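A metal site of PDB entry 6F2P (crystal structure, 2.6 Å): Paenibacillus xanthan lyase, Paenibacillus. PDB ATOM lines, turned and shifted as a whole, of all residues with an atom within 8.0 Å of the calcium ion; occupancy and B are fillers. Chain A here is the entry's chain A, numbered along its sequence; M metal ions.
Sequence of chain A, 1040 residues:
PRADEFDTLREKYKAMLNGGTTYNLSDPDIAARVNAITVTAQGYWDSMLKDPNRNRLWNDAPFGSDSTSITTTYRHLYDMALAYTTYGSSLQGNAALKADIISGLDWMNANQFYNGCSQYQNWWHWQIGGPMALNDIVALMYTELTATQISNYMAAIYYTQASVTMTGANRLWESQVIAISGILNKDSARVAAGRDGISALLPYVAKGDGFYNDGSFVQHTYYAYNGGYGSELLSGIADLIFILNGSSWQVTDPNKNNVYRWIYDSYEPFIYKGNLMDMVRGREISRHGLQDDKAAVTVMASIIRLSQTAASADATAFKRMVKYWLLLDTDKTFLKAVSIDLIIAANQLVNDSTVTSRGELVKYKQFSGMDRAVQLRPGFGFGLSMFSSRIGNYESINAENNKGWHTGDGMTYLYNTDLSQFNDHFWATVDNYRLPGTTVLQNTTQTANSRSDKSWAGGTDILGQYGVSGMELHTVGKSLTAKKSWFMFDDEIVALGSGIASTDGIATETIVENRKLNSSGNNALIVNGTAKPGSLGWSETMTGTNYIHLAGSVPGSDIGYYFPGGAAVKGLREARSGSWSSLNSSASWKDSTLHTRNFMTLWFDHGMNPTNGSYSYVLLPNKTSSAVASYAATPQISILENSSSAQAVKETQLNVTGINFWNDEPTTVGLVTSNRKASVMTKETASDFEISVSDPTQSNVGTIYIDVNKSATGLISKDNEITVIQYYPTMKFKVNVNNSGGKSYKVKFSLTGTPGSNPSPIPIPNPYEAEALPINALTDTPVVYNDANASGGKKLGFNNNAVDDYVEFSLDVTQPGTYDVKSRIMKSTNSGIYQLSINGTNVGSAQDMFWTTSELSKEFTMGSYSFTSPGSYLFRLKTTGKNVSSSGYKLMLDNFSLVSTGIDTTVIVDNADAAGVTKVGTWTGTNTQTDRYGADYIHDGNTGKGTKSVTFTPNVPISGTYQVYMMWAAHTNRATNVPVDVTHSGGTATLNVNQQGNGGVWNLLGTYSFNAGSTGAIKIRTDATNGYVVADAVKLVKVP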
ATOM      1  N   PRO A 767     -19.004  12.532 -10.478  1.00  0.00           N
ATOM      2  CA  PRO A 767     -17.598  12.879 -10.225  1.00  0.00           C
ATOM      3  C   PRO A 767     -17.398  14.378 -10.012  1.00  0.00           C
ATOM      4  O   PRO A 767     -18.235  15.175 -10.450  1.00  0.00           O
ATOM      5  CB  PRO A 767     -16.908  12.437 -11.526  1.00  0.00           C
ATOM      6  CG  PRO A 767     -17.944  12.679 -12.573  1.00  0.00           C
ATOM      7  CD  PRO A 767     -19.295  12.414 -11.917  1.00  0.00           C
ATOM      8  N   TYR A 768     -16.320  14.751  -9.339  1.00  0.00           N
ATOM      9  CA  TYR A 768     -15.964  16.148  -9.183  1.00  0.00           C
ATOM     10  C   TYR A 768     -15.157  16.525 -10.424  1.00  0.00           C
ATOM     11  O   TYR A 768     -13.974  16.200 -10.518  1.00  0.00           O
ATOM     12  CB  TYR A 768     -15.053  16.331  -7.970  1.00  0.00           C
ATOM     13  CG  TYR A 768     -15.698  16.130  -6.610  1.00  0.00           C
ATOM     14  CD1 TYR A 768     -15.780  14.875  -6.024  1.00  0.00           C
ATOM     15  CD2 TYR A 768     -16.166  17.219  -5.883  1.00  0.00           C
ATOM     16  CE1 TYR A 768     -16.345  14.696  -4.779  1.00  0.00           C
ATOM     17  CE2 TYR A 768     -16.733  17.054  -4.638  1.00  0.00           C
ATOM     18  CZ  TYR A 768     -16.827  15.788  -4.090  1.00  0.00           C
ATOM     19  OH  TYR A 768     -17.388  15.631  -2.846  1.00  0.00           O
ATOM     20  N   GLU A 769     -15.784  17.205 -11.382  1.00  0.00           N
ATOM     21  CA  GLU A 769     -15.097  17.544 -12.634  1.00  0.00           C
ATOM     22  C   GLU A 769     -13.989  18.562 -12.425  1.00  0.00           C
ATOM     23  O   GLU A 769     -14.239  19.672 -11.953  1.00  0.00           O
ATOM     24  CB  GLU A 769     -16.082  18.050 -13.682  1.00  0.00           C
ATOM     25  CG  GLU A 769     -17.212  17.076 -13.950  1.00  0.00           C
ATOM     26  CD  GLU A 769     -16.772  15.867 -14.768  1.00  0.00           C
ATOM     27  OE1 GLU A 769     -17.658  15.121 -15.226  1.00  0.00           O
ATOM     28  OE2 GLU A 769     -15.549  15.673 -14.966  1.00  0.00           O
ATOM     29  N   ALA A 770     -12.774  18.183 -12.784  1.00  0.00           N
ATOM     30  CA  ALA A 770     -11.603  19.023 -12.605  1.00  0.00           C
ATOM     31  C   ALA A 770     -11.809  20.378 -13.286  1.00  0.00           C
ATOM     32  O   ALA A 770     -11.486  21.414 -12.722  1.00  0.00           O
ATOM     33  CB  ALA A 770     -10.363  18.340 -13.163  1.00  0.00           C
ATOM     34  N   GLU A 771     -12.377  20.344 -14.487  1.00  0.00           N
ATOM     35  CA  GLU A 771     -12.600  21.558 -15.259  1.00  0.00           C
ATOM     36  C   GLU A 771     -13.559  22.541 -14.586  1.00  0.00           C
ATOM     37  O   GLU A 771     -13.716  23.667 -15.050  1.00  0.00           O
ATOM     38  CB  GLU A 771     -13.134  21.215 -16.651  1.00  0.00           C
ATOM     39  CG  GLU A 771     -14.522  20.579 -16.657  1.00  0.00           C
ATOM     40  CD  GLU A 771     -14.473  19.061 -16.764  1.00  0.00           C
ATOM     41  OE1 GLU A 771     -15.478  18.450 -17.171  1.00  0.00           O
ATOM     42  OE2 GLU A 771     -13.408  18.491 -16.432  1.00  0.00           O
ATOM     43  N   ALA A 772     -14.235  22.126 -13.514  1.00  0.00           N
ATOM     44  CA  ALA A 772     -15.206  22.999 -12.874  1.00  0.00           C
ATOM     45  C   ALA A 772     -14.932  23.188 -11.386  1.00  0.00           C
ATOM     46  O   ALA A 772     -15.800  23.636 -10.626  1.00  0.00           O
ATOM     47  CB  ALA A 772     -16.622  22.488 -13.096  1.00  0.00           C
ATOM     48  N   VAL A 784      -8.162  24.223 -19.682  1.00  0.00           N
ATOM     49  CA  VAL A 784      -9.164  23.209 -19.998  1.00  0.00           C
ATOM     50  C   VAL A 784      -9.180  22.913 -21.497  1.00  0.00           C
ATOM     51  O   VAL A 784      -9.262  23.823 -22.324  1.00  0.00           O
ATOM     52  CB  VAL A 784     -10.572  23.657 -19.564  1.00  0.00           C
ATOM     53  CG1 VAL A 784     -11.618  22.674 -20.047  1.00  0.00           C
ATOM     54  CG2 VAL A 784     -10.645  23.820 -18.055  1.00  0.00           C
ATOM     55  N   TYR A 785      -9.100  21.633 -21.854  1.00  0.00           N
ATOM     56  CA  TYR A 785      -9.220  21.219 -23.241  1.00  0.00           C
ATOM     57  C   TYR A 785     -10.470  20.360 -23.438  1.00  0.00           C
ATOM     58  O   TYR A 785     -10.915  19.673 -22.506  1.00  0.00           O
ATOM     59  CB  TYR A 785      -7.999  20.431 -23.679  1.00  0.00           C
ATOM     60  CG  TYR A 785      -6.706  21.192 -23.575  1.00  0.00           C
ATOM     61  CD1 TYR A 785      -6.359  22.136 -24.537  1.00  0.00           C
ATOM     62  CD2 TYR A 785      -5.825  20.979 -22.528  1.00  0.00           C
ATOM     63  CE1 TYR A 785      -5.171  22.847 -24.455  1.00  0.00           C
ATOM     64  CE2 TYR A 785      -4.627  21.670 -22.436  1.00  0.00           C
ATOM     65  CZ  TYR A 785      -4.308  22.610 -23.403  1.00  0.00           C
ATOM     66  OH  TYR A 785      -3.127  23.312 -23.320  1.00  0.00           O
ATOM     67  N   ASP A 787     -12.558  17.163 -25.116  1.00  0.00           N
ATOM     68  CA  ASP A 787     -12.229  15.764 -25.371  1.00  0.00           C
ATOM     69  C   ASP A 787     -13.465  14.915 -25.135  1.00  0.00           C
ATOM     70  O   ASP A 787     -13.934  14.795 -24.008  1.00  0.00           O
ATOM     71  CB  ASP A 787     -11.084  15.319 -24.451  1.00  0.00           C
ATOM     72  CG  ASP A 787     -10.516  13.949 -24.813  1.00  0.00           C
ATOM     73  OD1 ASP A 787     -11.263  13.119 -25.378  1.00  0.00           O
ATOM     74  OD2 ASP A 787      -9.323  13.703 -24.538  1.00  0.00           O
ATOM     75  N   ASN A 789     -13.776  11.861 -25.025  1.00  0.00           N
ATOM     76  CA  ASN A 789     -13.486  10.694 -24.194  1.00  0.00           C
ATOM     77  C   ASN A 789     -13.410  11.019 -22.705  1.00  0.00           C
ATOM     78  O   ASN A 789     -13.230  10.123 -21.883  1.00  0.00           O
ATOM     79  CB  ASN A 789     -12.173  10.055 -24.613  1.00  0.00           C
ATOM     80  CG  ASN A 789     -12.178   9.548 -26.032  1.00  0.00           C
ATOM     81  OD1 ASN A 789     -11.233   9.775 -26.779  1.00  0.00           O
ATOM     82  ND2 ASN A 789     -13.259   8.850 -26.404  1.00  0.00           N
ATOM     83  N   ALA A 790     -13.517  12.302 -22.375  1.00  0.00           N
ATOM     84  CA  ALA A 790     -13.385  12.732 -20.990  1.00  0.00           C
ATOM     85  C   ALA A 790     -14.744  12.936 -20.358  1.00  0.00           C
ATOM     86  O   ALA A 790     -15.718  13.292 -21.036  1.00  0.00           O
ATOM     87  CB  ALA A 790     -12.568  13.998 -20.915  1.00  0.00           C
ATOM     88  N   SER A 791     -14.794  12.695 -19.053  1.00  0.00           N
ATOM     89  CA  SER A 791     -15.972  12.966 -18.259  1.00  0.00           C
ATOM     90  C   SER A 791     -16.354  14.444 -18.385  1.00  0.00           C
ATOM     91  O   SER A 791     -15.541  15.337 -18.137  1.00  0.00           O
ATOM     92  CB  SER A 791     -15.676  12.642 -16.797  1.00  0.00           C
ATOM     93  OG  SER A 791     -16.867  12.538 -16.041  1.00  0.00           O
ATOM     94  N   GLY A 792     -17.597  14.693 -18.794  1.00  0.00           N
ATOM     95  CA  GLY A 792     -18.069  16.050 -18.992  1.00  0.00           C
ATOM     96  C   GLY A 792     -17.562  16.669 -20.283  1.00  0.00           C
ATOM     97  O   GLY A 792     -17.819  17.838 -20.562  1.00  0.00           O
ATOM     98  N   GLY A 793     -16.839  15.871 -21.064  1.00  0.00           N
ATOM     99  CA  GLY A 793     -16.323  16.320 -22.347  1.00  0.00           C
ATOM    100  C   GLY A 793     -15.176  17.299 -22.203  1.00  0.00           C
ATOM    101  O   GLY A 793     -14.775  17.935 -23.176  1.00  0.00           O
ATOM    102  N   LYS A 794     -14.639  17.422 -20.992  1.00  0.00           N
ATOM    103  CA  LYS A 794     -13.540  18.340 -20.736  1.00  0.00           C
ATOM    104  C   LYS A 794     -12.507  17.730 -19.801  1.00  0.00           C
ATOM    105  O   LYS A 794     -12.838  16.979 -18.892  1.00  0.00           O
ATOM    106  CB  LYS A 794     -14.053  19.653 -20.156  1.00  0.00           C
ATOM    107  CG  LYS A 794     -14.964  20.452 -21.079  1.00  0.00           C
ATOM    108  CD  LYS A 794     -15.464  21.720 -20.407  1.00  0.00           C
ATOM    109  CE  LYS A 794     -16.299  22.557 -21.364  1.00  0.00           C
ATOM    110  NZ  LYS A 794     -15.512  22.968 -22.563  1.00  0.00           N
ATOM    111  N   LYS A 795     -11.246  18.054 -20.042  1.00  0.00           N
ATOM    112  CA  LYS A 795     -10.174  17.648 -19.144  1.00  0.00           C
ATOM    113  C   LYS A 795      -9.349  18.883 -18.754  1.00  0.00           C
ATOM    114  O   LYS A 795      -9.383  19.904 -19.452  1.00  0.00           O
ATOM    115  CB  LYS A 795      -9.297  16.590 -19.811  1.00  0.00           C
ATOM    116  CG  LYS A 795      -8.640  17.058 -21.096  1.00  0.00           C
ATOM    117  CD  LYS A 795      -8.057  15.918 -21.918  1.00  0.00           C
ATOM    118  CE  LYS A 795      -7.397  16.453 -23.176  1.00  0.00           C
ATOM    119  NZ  LYS A 795      -7.316  15.435 -24.246  1.00  0.00           N
ATOM    120  N   LEU A 796      -8.619  18.794 -17.641  1.00  0.00           N
ATOM    121  CA  LEU A 796      -7.797  19.916 -17.184  1.00  0.00           C
ATOM    122  C   LEU A 796      -6.324  19.621 -17.392  1.00  0.00           C
ATOM    123  O   LEU A 796      -5.768  18.712 -16.766  1.00  0.00           O
ATOM    124  CB  LEU A 796      -8.070  20.236 -15.715  1.00  0.00           C
ATOM    125  CG  LEU A 796      -7.426  21.534 -15.231  1.00  0.00           C
ATOM    126  CD1 LEU A 796      -7.937  22.693 -16.050  1.00  0.00           C
ATOM    127  CD2 LEU A 796      -7.651  21.783 -13.744  1.00  0.00           C
ATOM    128  N   ARG A 824      -9.518  10.339 -12.456  1.00  0.00           N
ATOM    129  CA  ARG A 824      -9.519   9.848 -13.836  1.00  0.00           C
ATOM    130  C   ARG A 824      -8.582  10.715 -14.647  1.00  0.00           C
ATOM    131  O   ARG A 824      -8.756  11.931 -14.718  1.00  0.00           O
ATOM    132  CB  ARG A 824     -10.931   9.854 -14.431  1.00  0.00           C
ATOM    133  CG  ARG A 824     -11.026   9.208 -15.809  1.00  0.00           C
ATOM    134  CD  ARG A 824     -12.467   9.162 -16.305  1.00  0.00           C
ATOM    135  NE  ARG A 824     -12.699   8.062 -17.233  1.00  0.00           N
ATOM    136  CZ  ARG A 824     -12.867   8.201 -18.542  1.00  0.00           C
ATOM    137  NH1 ARG A 824     -12.838   9.401 -19.097  1.00  0.00           N
ATOM    138  NH2 ARG A 824     -13.080   7.139 -19.304  1.00  0.00           N
ATOM    139  N   MET A 826      -6.561  11.450 -18.300  1.00  0.00           N
ATOM    140  CA  MET A 826      -6.489  11.211 -19.734  1.00  0.00           C
ATOM    141  C   MET A 826      -5.035  10.970 -20.155  1.00  0.00           C
ATOM    142  O   MET A 826      -4.110  11.533 -19.562  1.00  0.00           O
ATOM    143  CB  MET A 826      -7.075  12.396 -20.503  1.00  0.00           C
ATOM    144  CG  MET A 826      -8.474  12.759 -20.087  1.00  0.00           C
ATOM    145  SD  MET A 826      -9.644  11.480 -20.555  1.00  0.00           S
ATOM    146  CE  MET A 826     -10.066  10.862 -18.942  1.00  0.00           C
ATOM    147  N   LEU A 893      -5.879  16.038 -16.190  1.00  0.00           N
ATOM    148  CA  LEU A 893      -6.803  15.631 -15.132  1.00  0.00           C
ATOM    149  C   LEU A 893      -8.268  15.727 -15.572  1.00  0.00           C
ATOM    150  O   LEU A 893      -8.732  16.792 -15.978  1.00  0.00           O
ATOM    151  CB  LEU A 893      -6.553  16.480 -13.889  1.00  0.00           C
ATOM    152  CG  LEU A 893      -7.411  16.282 -12.640  1.00  0.00           C
ATOM    153  CD1 LEU A 893      -7.390  14.845 -12.151  1.00  0.00           C
ATOM    154  CD2 LEU A 893      -6.900  17.212 -11.551  1.00  0.00           C
ATOM    155  N   ASP A 894      -8.999  14.615 -15.476  1.00  0.00           N
ATOM    156  CA  ASP A 894     -10.405  14.620 -15.889  1.00  0.00           C
ATOM    157  C   ASP A 894     -11.315  14.905 -14.700  1.00  0.00           C
ATOM    158  O   ASP A 894     -12.138  15.818 -14.751  1.00  0.00           O
ATOM    159  CB  ASP A 894     -10.787  13.293 -16.571  1.00  0.00           C
ATOM    160  CG  ASP A 894     -12.198  13.334 -17.178  1.00  0.00           C
ATOM    161  OD1 ASP A 894     -12.843  14.402 -17.162  1.00  0.00           O
ATOM    162  OD2 ASP A 894     -12.655  12.281 -17.692  1.00  0.00           O
ATOM    163  N   ASN A 895     -11.169  14.112 -13.636  1.00  0.00           N
ATOM    164  CA  ASN A 895     -12.002  14.301 -12.452  1.00  0.00           C
ATOM    165  C   ASN A 895     -11.472  13.603 -11.196  1.00  0.00           C
ATOM    166  O   ASN A 895     -10.437  12.946 -11.230  1.00  0.00           O
ATOM    167  CB  ASN A 895     -13.453  13.883 -12.725  1.00  0.00           C
ATOM    168  CG  ASN A 895     -13.615  12.393 -13.015  1.00  0.00           C
ATOM    169  OD1 ASN A 895     -12.835  11.568 -12.547  1.00  0.00           O
ATOM    170  ND2 ASN A 895     -14.634  12.061 -13.789  1.00  0.00           N
ATOM    171  N   PHE A 896     -12.194  13.783 -10.099  1.00  0.00           N
ATOM    172  CA  PHE A 896     -11.984  13.004  -8.883  1.00  0.00           C
ATOM    173  C   PHE A 896     -13.268  12.250  -8.594  1.00  0.00           C
ATOM    174  O   PHE A 896     -14.356  12.679  -8.966  1.00  0.00           O
ATOM    175  CB  PHE A 896     -11.671  13.910  -7.692  1.00  0.00           C
ATOM    176  CG  PHE A 896     -10.334  14.586  -7.751  1.00  0.00           C
ATOM    177  CD1 PHE A 896      -9.174  13.885  -7.477  1.00  0.00           C
ATOM    178  CD2 PHE A 896     -10.235  15.940  -8.042  1.00  0.00           C
ATOM    179  CE1 PHE A 896      -7.942  14.490  -7.527  1.00  0.00           C
ATOM    180  CE2 PHE A 896      -8.998  16.567  -8.084  1.00  0.00           C
ATOM    181  CZ  PHE A 896      -7.844  15.844  -7.828  1.00  0.00           C
HETATM  182 CA    CA M   1     -13.961  16.344 -16.832  1.00  0.00          CA
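Five residues have an atom within 4 Å of the calcium ion: Glu 769, Glu 771, Ser 791, Lys 794 and Asp 894.
Along chain A the residues within 4 Å of the calcium ion span positions 769 to 894.
The calcium ion is bound by the side-chain carboxylate (OE2) of Glu 771, the side-chain carboxylate (OD1) of Asp 894, the backbone carbonyl oxygen (O) of Ser 791, the backbone carbonyl oxygen (O) of Lys 794, the side-chain carboxylate (OE2) of Glu 769, the side-chain carboxylate (OE1) of Glu 771 and the backbone carbonyl oxygen (O) of Asp 894.
The side-chain carboxylate (OD2) of Asp 894 lies within salt-bridge range of the guanidinium group (NH1) of Arg 824.
The backbone carbonyl oxygen (O) of Asp 894 sits close to the backbone NH (N) of Ala 770 (3.1 Å).
The side-chain hydroxyl (OG) of Ser 791 lies within hydrogen-bond range of the side-chain amide nitrogen (ND2) of Asn 895 (3.2 Å).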
